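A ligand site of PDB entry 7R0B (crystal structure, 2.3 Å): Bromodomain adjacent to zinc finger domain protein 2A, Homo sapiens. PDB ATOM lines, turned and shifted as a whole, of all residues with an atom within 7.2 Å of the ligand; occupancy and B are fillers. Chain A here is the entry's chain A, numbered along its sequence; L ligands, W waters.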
ATOM      1  N   TRP A  23       7.346  -8.534  -5.762  1.00  0.00           N
ATOM      2  CA  TRP A  23       8.798  -8.441  -5.574  1.00  0.00           C
ATOM      3  C   TRP A  23       9.266  -7.321  -4.648  1.00  0.00           C
ATOM      4  O   TRP A  23      10.272  -7.537  -3.949  1.00  0.00           O
ATOM      5  CB  TRP A  23       9.498  -8.345  -6.941  1.00  0.00           C
ATOM      6  CG  TRP A  23       9.030  -7.230  -7.799  1.00  0.00           C
ATOM      7  CD1 TRP A  23       8.051  -7.271  -8.729  1.00  0.00           C
ATOM      8  CD2 TRP A  23       9.544  -5.882  -7.817  1.00  0.00           C
ATOM      9  NE1 TRP A  23       7.910  -6.046  -9.340  1.00  0.00           N
ATOM     10  CE2 TRP A  23       8.811  -5.169  -8.785  1.00  0.00           C
ATOM     11  CE3 TRP A  23      10.555  -5.227  -7.122  1.00  0.00           C
ATOM     12  CZ2 TRP A  23       9.050  -3.825  -9.070  1.00  0.00           C
ATOM     13  CZ3 TRP A  23      10.783  -3.884  -7.397  1.00  0.00           C
ATOM     14  CH2 TRP A  23      10.035  -3.205  -8.362  1.00  0.00           C
ATOM     15  N   PRO A  24       8.633  -6.141  -4.549  1.00  0.00           N
ATOM     16  CA  PRO A  24       9.128  -5.145  -3.602  1.00  0.00           C
ATOM     17  C   PRO A  24       8.805  -5.456  -2.155  1.00  0.00           C
ATOM     18  O   PRO A  24       9.347  -4.782  -1.271  1.00  0.00           O
ATOM     19  CB  PRO A  24       8.410  -3.838  -4.027  1.00  0.00           C
ATOM     20  CG  PRO A  24       7.745  -4.153  -5.323  1.00  0.00           C
ATOM     21  CD  PRO A  24       7.485  -5.612  -5.313  1.00  0.00           C
ATOM     22  N   PHE A  25       7.935  -6.420  -1.873  1.00  0.00           N
ATOM     23  CA  PHE A  25       7.427  -6.557  -0.516  1.00  0.00           C
ATOM     24  C   PHE A  25       7.751  -7.898   0.123  1.00  0.00           C
ATOM     25  O   PHE A  25       7.225  -8.207   1.194  1.00  0.00           O
ATOM     26  CB  PHE A  25       5.907  -6.330  -0.505  1.00  0.00           C
ATOM     27  CG  PHE A  25       5.472  -5.196  -1.388  1.00  0.00           C
ATOM     28  CD1 PHE A  25       5.624  -3.885  -0.986  1.00  0.00           C
ATOM     29  CD2 PHE A  25       4.898  -5.449  -2.611  1.00  0.00           C
ATOM     30  CE1 PHE A  25       5.223  -2.845  -1.784  1.00  0.00           C
ATOM     31  CE2 PHE A  25       4.490  -4.394  -3.427  1.00  0.00           C
ATOM     32  CZ  PHE A  25       4.655  -3.094  -3.000  1.00  0.00           C
ATOM     33  N   LEU A  26       8.628  -8.709  -0.477  1.00  0.00           N
ATOM     34  CA  LEU A  26       8.902 -10.016   0.098  1.00  0.00           C
ATOM     35  C   LEU A  26       9.845  -9.941   1.299  1.00  0.00           C
ATOM     36  O   LEU A  26       9.953 -10.919   2.037  1.00  0.00           O
ATOM     37  CB  LEU A  26       9.475 -10.952  -0.977  1.00  0.00           C
ATOM     38  CG  LEU A  26       8.512 -11.287  -2.121  1.00  0.00           C
ATOM     39  CD1 LEU A  26       9.166 -12.200  -3.135  1.00  0.00           C
ATOM     40  CD2 LEU A  26       7.248 -11.930  -1.579  1.00  0.00           C
ATOM     41  N   GLU A  27      10.515  -8.819   1.514  1.00  0.00           N
ATOM     42  CA  GLU A  27      11.456  -8.685   2.609  1.00  0.00           C
ATOM     43  C   GLU A  27      11.437  -7.233   3.074  1.00  0.00           C
ATOM     44  O   GLU A  27      11.047  -6.341   2.311  1.00  0.00           O
ATOM     45  CB  GLU A  27      12.877  -9.106   2.177  1.00  0.00           C
ATOM     46  CG  GLU A  27      13.482  -8.300   1.045  1.00  0.00           C
ATOM     47  CD  GLU A  27      14.928  -8.690   0.760  1.00  0.00           C
ATOM     48  OE1 GLU A  27      15.849  -7.975   1.221  1.00  0.00           O
ATOM     49  OE2 GLU A  27      15.149  -9.726   0.091  1.00  0.00           O
ATOM     50  N   PRO A  28      11.817  -6.965   4.324  1.00  0.00           N
ATOM     51  CA  PRO A  28      11.830  -5.587   4.820  1.00  0.00           C
ATOM     52  C   PRO A  28      12.713  -4.695   3.963  1.00  0.00           C
ATOM     53  O   PRO A  28      13.742  -5.128   3.441  1.00  0.00           O
ATOM     54  CB  PRO A  28      12.383  -5.706   6.240  1.00  0.00           C
ATOM     55  CG  PRO A  28      12.250  -7.148   6.595  1.00  0.00           C
ATOM     56  CD  PRO A  28      12.392  -7.896   5.314  1.00  0.00           C
ATOM     57  N   VAL A  29      12.310  -3.436   3.846  1.00  0.00           N
ATOM     58  CA  VAL A  29      13.178  -2.454   3.223  1.00  0.00           C
ATOM     59  C   VAL A  29      14.426  -2.295   4.068  1.00  0.00           C
ATOM     60  O   VAL A  29      14.355  -2.222   5.301  1.00  0.00           O
ATOM     61  CB  VAL A  29      12.445  -1.112   3.050  1.00  0.00           C
ATOM     62  CG1 VAL A  29      13.399  -0.066   2.517  1.00  0.00           C
ATOM     63  CG2 VAL A  29      11.247  -1.293   2.132  1.00  0.00           C
ATOM     64  N   ASN A  30      15.582  -2.289   3.419  1.00  0.00           N
ATOM     65  CA  ASN A  30      16.845  -2.055   4.063  1.00  0.00           C
ATOM     66  C   ASN A  30      17.130  -0.553   4.063  1.00  0.00           C
ATOM     67  O   ASN A  30      17.496  -0.010   3.019  1.00  0.00           O
ATOM     68  CB  ASN A  30      17.966  -2.829   3.346  1.00  0.00           C
ATOM     69  CG  ASN A  30      19.278  -2.749   4.067  1.00  0.00           C
ATOM     70  OD1 ASN A  30      19.506  -1.849   4.868  1.00  0.00           O
ATOM     71  ND2 ASN A  30      20.172  -3.700   3.797  1.00  0.00           N
ATOM     72  N   LEU A  33      20.011   1.148   2.339  1.00  0.00           N
ATOM     73  CA  LEU A  33      19.970   1.218   0.885  1.00  0.00           C
ATOM     74  C   LEU A  33      18.972   2.235   0.352  1.00  0.00           C
ATOM     75  O   LEU A  33      18.999   2.548  -0.843  1.00  0.00           O
ATOM     76  CB  LEU A  33      19.637  -0.169   0.306  1.00  0.00           C
ATOM     77  CG  LEU A  33      20.531  -1.292   0.833  1.00  0.00           C
ATOM     78  CD1 LEU A  33      20.111  -2.681   0.317  1.00  0.00           C
ATOM     79  CD2 LEU A  33      21.984  -1.014   0.491  1.00  0.00           C
ATOM     80  N   VAL A  34      18.103   2.778   1.208  1.00  0.00           N
ATOM     81  CA  VAL A  34      17.010   3.642   0.761  1.00  0.00           C
ATOM     82  C   VAL A  34      17.101   4.932   1.561  1.00  0.00           C
ATOM     83  O   VAL A  34      16.620   5.007   2.696  1.00  0.00           O
ATOM     84  CB  VAL A  34      15.642   2.956   0.927  1.00  0.00           C
ATOM     85  CG1 VAL A  34      14.538   3.867   0.418  1.00  0.00           C
ATOM     86  CG2 VAL A  34      15.621   1.634   0.172  1.00  0.00           C
ATOM     87  N   SER A  35      17.739   5.948   0.970  1.00  0.00           N
ATOM     88  CA  SER A  35      17.851   7.242   1.635  1.00  0.00           C
ATOM     89  C   SER A  35      16.464   7.775   1.942  1.00  0.00           C
ATOM     90  O   SER A  35      15.594   7.826   1.066  1.00  0.00           O
ATOM     91  CB  SER A  35      18.613   8.225   0.754  1.00  0.00           C
ATOM     92  OG  SER A  35      19.667   7.590   0.056  1.00  0.00           O
ATOM     93  N   TYR A  37      14.211   6.481   4.172  1.00  0.00           N
ATOM     94  CA  TYR A  37      13.147   5.548   4.515  1.00  0.00           C
ATOM     95  C   TYR A  37      12.835   5.604   6.008  1.00  0.00           C
ATOM     96  O   TYR A  37      11.663   5.708   6.402  1.00  0.00           O
ATOM     97  CB  TYR A  37      13.522   4.120   4.121  1.00  0.00           C
ATOM     98  CG  TYR A  37      12.318   3.217   4.087  1.00  0.00           C
ATOM     99  CD1 TYR A  37      11.448   3.255   3.017  1.00  0.00           C
ATOM    100  CD2 TYR A  37      12.052   2.324   5.124  1.00  0.00           C
ATOM    101  CE1 TYR A  37      10.340   2.457   2.969  1.00  0.00           C
ATOM    102  CE2 TYR A  37      10.931   1.492   5.079  1.00  0.00           C
ATOM    103  CZ  TYR A  37      10.074   1.573   3.986  1.00  0.00           C
ATOM    104  OH  TYR A  37       8.946   0.776   3.883  1.00  0.00           O
ATOM    105  N   ILE A  41       9.052   6.509   7.108  1.00  0.00           N
ATOM    106  CA  ILE A  41       8.159   5.388   7.387  1.00  0.00           C
ATOM    107  C   ILE A  41       8.323   5.021   8.855  1.00  0.00           C
ATOM    108  O   ILE A  41       9.326   4.426   9.261  1.00  0.00           O
ATOM    109  CB  ILE A  41       8.461   4.206   6.460  1.00  0.00           C
ATOM    110  CG1 ILE A  41       8.027   4.540   5.027  1.00  0.00           C
ATOM    111  CG2 ILE A  41       7.741   2.929   6.901  1.00  0.00           C
ATOM    112  CD1 ILE A  41       6.595   4.998   4.939  1.00  0.00           C
ATOM    113  N   MET A  45       6.630  -2.570   7.336  1.00  0.00           N
ATOM    114  CA  MET A  45       5.937  -3.842   7.287  1.00  0.00           C
ATOM    115  C   MET A  45       6.183  -4.463   5.928  1.00  0.00           C
ATOM    116  O   MET A  45       6.363  -3.757   4.932  1.00  0.00           O
ATOM    117  CB  MET A  45       4.444  -3.671   7.570  1.00  0.00           C
ATOM    118  CG  MET A  45       3.655  -4.965   7.603  1.00  0.00           C
ATOM    119  SD  MET A  45       4.286  -6.158   8.787  1.00  0.00           S
ATOM    120  CE  MET A  45       4.356  -5.150  10.280  1.00  0.00           C
ATOM    121  N   ASP A  46       6.202  -5.795   5.898  1.00  0.00           N
ATOM    122  CA  ASP A  46       6.441  -6.523   4.652  1.00  0.00           C
ATOM    123  C   ASP A  46       5.830  -7.913   4.762  1.00  0.00           C
ATOM    124  O   ASP A  46       5.360  -8.314   5.825  1.00  0.00           O
ATOM    125  CB  ASP A  46       7.945  -6.574   4.346  1.00  0.00           C
ATOM    126  CG  ASP A  46       8.672  -7.492   5.284  1.00  0.00           C
ATOM    127  OD1 ASP A  46       8.874  -7.093   6.450  1.00  0.00           O
ATOM    128  OD2 ASP A  46       9.007  -8.610   4.855  1.00  0.00           O
ATOM    129  N   VAL A  72       1.463  -2.290   4.614  1.00  0.00           N
ATOM    130  CA  VAL A  72       2.444  -2.489   3.544  1.00  0.00           C
ATOM    131  C   VAL A  72       2.185  -1.506   2.411  1.00  0.00           C
ATOM    132  O   VAL A  72       3.103  -0.853   1.898  1.00  0.00           O
ATOM    133  CB  VAL A  72       2.393  -3.956   3.032  1.00  0.00           C
ATOM    134  CG1 VAL A  72       3.348  -4.131   1.868  1.00  0.00           C
ATOM    135  CG2 VAL A  72       2.741  -4.939   4.146  1.00  0.00           C
ATOM    136  N   ASN A  75       2.452   2.365   3.499  1.00  0.00           N
ATOM    137  CA  ASN A  75       3.867   2.752   3.472  1.00  0.00           C
ATOM    138  C   ASN A  75       4.343   2.916   2.039  1.00  0.00           C
ATOM    139  O   ASN A  75       5.060   3.862   1.712  1.00  0.00           O
ATOM    140  CB  ASN A  75       4.760   1.718   4.163  1.00  0.00           C
ATOM    141  CG  ASN A  75       4.494   1.608   5.644  1.00  0.00           C
ATOM    142  OD1 ASN A  75       3.900   2.488   6.235  1.00  0.00           O
ATOM    143  ND2 ASN A  75       4.919   0.506   6.242  1.00  0.00           N
ATOM    144  N   CYS A  76       3.924   1.993   1.171  1.00  0.00           N
ATOM    145  CA  CYS A  76       4.301   2.028  -0.244  1.00  0.00           C
ATOM    146  C   CYS A  76       3.847   3.312  -0.927  1.00  0.00           C
ATOM    147  O   CYS A  76       4.638   3.992  -1.592  1.00  0.00           O
ATOM    148  CB  CYS A  76       3.732   0.812  -0.969  1.00  0.00           C
ATOM    149  SG  CYS A  76       4.169   0.832  -2.701  1.00  0.00           S
ATOM    150  N   GLN A  77       2.562   3.662  -0.771  1.00  0.00           N
ATOM    151  CA  GLN A  77       2.078   4.932  -1.318  1.00  0.00           C
ATOM    152  C   GLN A  77       2.647   6.148  -0.593  1.00  0.00           C
ATOM    153  O   GLN A  77       2.688   7.238  -1.179  1.00  0.00           O
ATOM    154  CB  GLN A  77       0.562   4.989  -1.280  1.00  0.00           C
ATOM    155  CG  GLN A  77      -0.083   3.894  -2.083  1.00  0.00           C
ATOM    156  CD  GLN A  77      -1.573   3.862  -1.885  1.00  0.00           C
ATOM    157  OE1 GLN A  77      -2.320   4.598  -2.537  1.00  0.00           O
ATOM    158  NE2 GLN A  77      -2.025   2.997  -0.980  1.00  0.00           N
ATOM    159  N   PHE A  79       5.833   6.418   0.476  1.00  0.00           N
ATOM    160  CA  PHE A  79       7.218   6.642   0.108  1.00  0.00           C
ATOM    161  C   PHE A  79       7.465   6.723  -1.397  1.00  0.00           C
ATOM    162  O   PHE A  79       8.345   7.489  -1.829  1.00  0.00           O
ATOM    163  CB  PHE A  79       8.100   5.546   0.686  1.00  0.00           C
ATOM    164  CG  PHE A  79       9.550   5.903   0.676  1.00  0.00           C
ATOM    165  CD1 PHE A  79      10.101   6.630   1.722  1.00  0.00           C
ATOM    166  CD2 PHE A  79      10.346   5.563  -0.398  1.00  0.00           C
ATOM    167  CE1 PHE A  79      11.427   6.989   1.700  1.00  0.00           C
ATOM    168  CE2 PHE A  79      11.693   5.914  -0.419  1.00  0.00           C
ATOM    169  CZ  PHE A  79      12.232   6.623   0.634  1.00  0.00           C
ATOM    170  N   ASN A  80       6.753   5.959  -2.211  1.00  0.00           N
ATOM    171  CA  ASN A  80       7.014   5.880  -3.646  1.00  0.00           C
ATOM    172  C   ASN A  80       5.944   6.602  -4.448  1.00  0.00           C
ATOM    173  O   ASN A  80       4.753   6.521  -4.130  1.00  0.00           O
ATOM    174  CB  ASN A  80       7.072   4.431  -4.118  1.00  0.00           C
ATOM    175  CG  ASN A  80       7.973   3.582  -3.269  1.00  0.00           C
ATOM    176  OD1 ASN A  80       9.184   3.525  -3.479  1.00  0.00           O
ATOM    177  ND2 ASN A  80       7.374   2.911  -2.282  1.00  0.00           N
ATOM    178  N   SER A  84       6.130   5.284 -10.085  1.00  0.00           N
ATOM    179  CA  SER A  84       7.375   4.539  -9.970  1.00  0.00           C
ATOM    180  C   SER A  84       7.108   3.043 -10.120  1.00  0.00           C
ATOM    181  O   SER A  84       5.960   2.598 -10.042  1.00  0.00           O
ATOM    182  CB  SER A  84       8.053   4.813  -8.618  1.00  0.00           C
ATOM    183  OG  SER A  84       7.360   4.201  -7.542  1.00  0.00           O
ATOM    184  N   VAL A  86       8.021   0.649  -8.026  1.00  0.00           N
ATOM    185  CA  VAL A  86       7.528   0.115  -6.763  1.00  0.00           C
ATOM    186  C   VAL A  86       6.099   0.602  -6.536  1.00  0.00           C
ATOM    187  O   VAL A  86       5.216  -0.179  -6.151  1.00  0.00           O
ATOM    188  CB  VAL A  86       8.453   0.492  -5.596  1.00  0.00           C
ATOM    189  CG1 VAL A  86       7.784   0.186  -4.260  1.00  0.00           C
ATOM    190  CG2 VAL A  86       9.807  -0.249  -5.709  1.00  0.00           C
ATOM    191  N   GLY A  87       5.841   1.882  -6.819  1.00  0.00           N
ATOM    192  CA  GLY A  87       4.488   2.381  -6.709  1.00  0.00           C
ATOM    193  C   GLY A  87       3.496   1.576  -7.532  1.00  0.00           C
ATOM    194  O   GLY A  87       2.462   1.130  -7.029  1.00  0.00           O
HETATM  195  C1  LIG L   1      13.290  -2.216  -4.555  1.00  0.00           C
HETATM  196  C2  LIG L   1      12.570  -2.596  -3.377  1.00  0.00           C
HETATM  197  C3  LIG L   1      11.273   2.370  -0.413  1.00  0.00           C
HETATM  198  C4  LIG L   1      13.648  -4.623  -4.031  1.00  0.00           C
HETATM  199  C5  LIG L   1      14.201  -8.456  -4.877  1.00  0.00           C
HETATM  200  C6  LIG L   1      13.942  -6.973  -5.179  1.00  0.00           C
HETATM  201  C7  LIG L   1      12.458   1.621  -3.820  1.00  0.00           C
HETATM  202  C8  LIG L   1      12.918   0.618  -2.689  1.00  0.00           C
HETATM  203  C9  LIG L   1      11.760  -0.322  -2.218  1.00  0.00           C
HETATM  204  C10 LIG L   1      11.646  -1.676  -2.526  1.00  0.00           C
HETATM  205  C11 LIG L   1       9.871  -1.205  -1.255  1.00  0.00           C
HETATM  206  C12 LIG L   1       8.548  -1.398  -0.453  1.00  0.00           C
HETATM  207  C13 LIG L   1      10.642  -0.004  -1.420  1.00  0.00           C
HETATM  208  C14 LIG L   1      10.251   1.314  -0.786  1.00  0.00           C
HETATM  209  C15 LIG L   1      15.320  -8.055  -2.864  1.00  0.00           C
HETATM  210  C16 LIG L   1      14.779  -6.620  -2.795  1.00  0.00           C
HETATM  211  N1  LIG L   1      10.488  -2.159  -1.909  1.00  0.00           N
HETATM  212  N2  LIG L   1      12.781  -4.020  -3.083  1.00  0.00           N
HETATM  213  N3  LIG L   1      14.098  -6.049  -4.000  1.00  0.00           N
HETATM  214  N4  LIG L   1      15.415  -8.597  -4.185  1.00  0.00           N
HETATM  215  O1  LIG L   1       9.122   1.523  -0.550  1.00  0.00           O
HETATM  216  S1  LIG L   1      14.106  -3.521  -5.127  1.00  0.00           S
HETATM  217  O   HOH W   1       5.726  -1.053   1.561  1.00  0.00           O
HETATM  218  O   HOH W   2      12.410  -5.559  -0.238  1.00  0.00           O
HETATM  219  O   HOH W   3       7.566   1.274   1.369  1.00  0.00           O
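O1 of the ligand sits at hydrogen-bond distance from ND2 of Asn 80. The backbone carbonyl oxygen of Pro 24 sits at hydrogen-bond distance from a nitrogen (N1) of the ligand (2.9 Å).
ND2 of Asn 80 sits at hydrogen-bond distance from O of Cys 76, 3.0 Å away. The side-chain sulfur (SG) of Cys 76 sits at hydrogen-bond distance from the backbone carbonyl oxygen (O) of Val 86 (3.7 Å).
Trp 23 touches the ligand (O to C6, 3.9 Å). CE1 of Phe 25 touches C12 of the ligand, at 3.9 Å. OE2 of Glu 27 touches C15 of the ligand, at 3.4 Å. Val 29 touches the ligand (CG2 to C11, 3.7 Å). Val 34 touches the ligand. Tyr 37 touches the ligand (CE1 to C3, 3.5 Å). Phe 79 touches the ligand. Val 86 touches the ligand (CG2 to C7, 3.8 Å). Ten residues have an atom within 4 Å of the ligand: Trp 23, Pro 24, Phe 25, Glu 27, Val 29, Val 34, Tyr 37, Phe 79, Asn 80 and Val 86. Along chain A the residues within 4 Å of the ligand span positions 23 to 86.
Water W3 bridges O1 of the ligand (2.5 Å) and OH of Tyr 37 (2.9 Å). Water W2 lies within hydrogen-bond range of O of Glu 27, N2 of the ligand and O of Pro 24.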
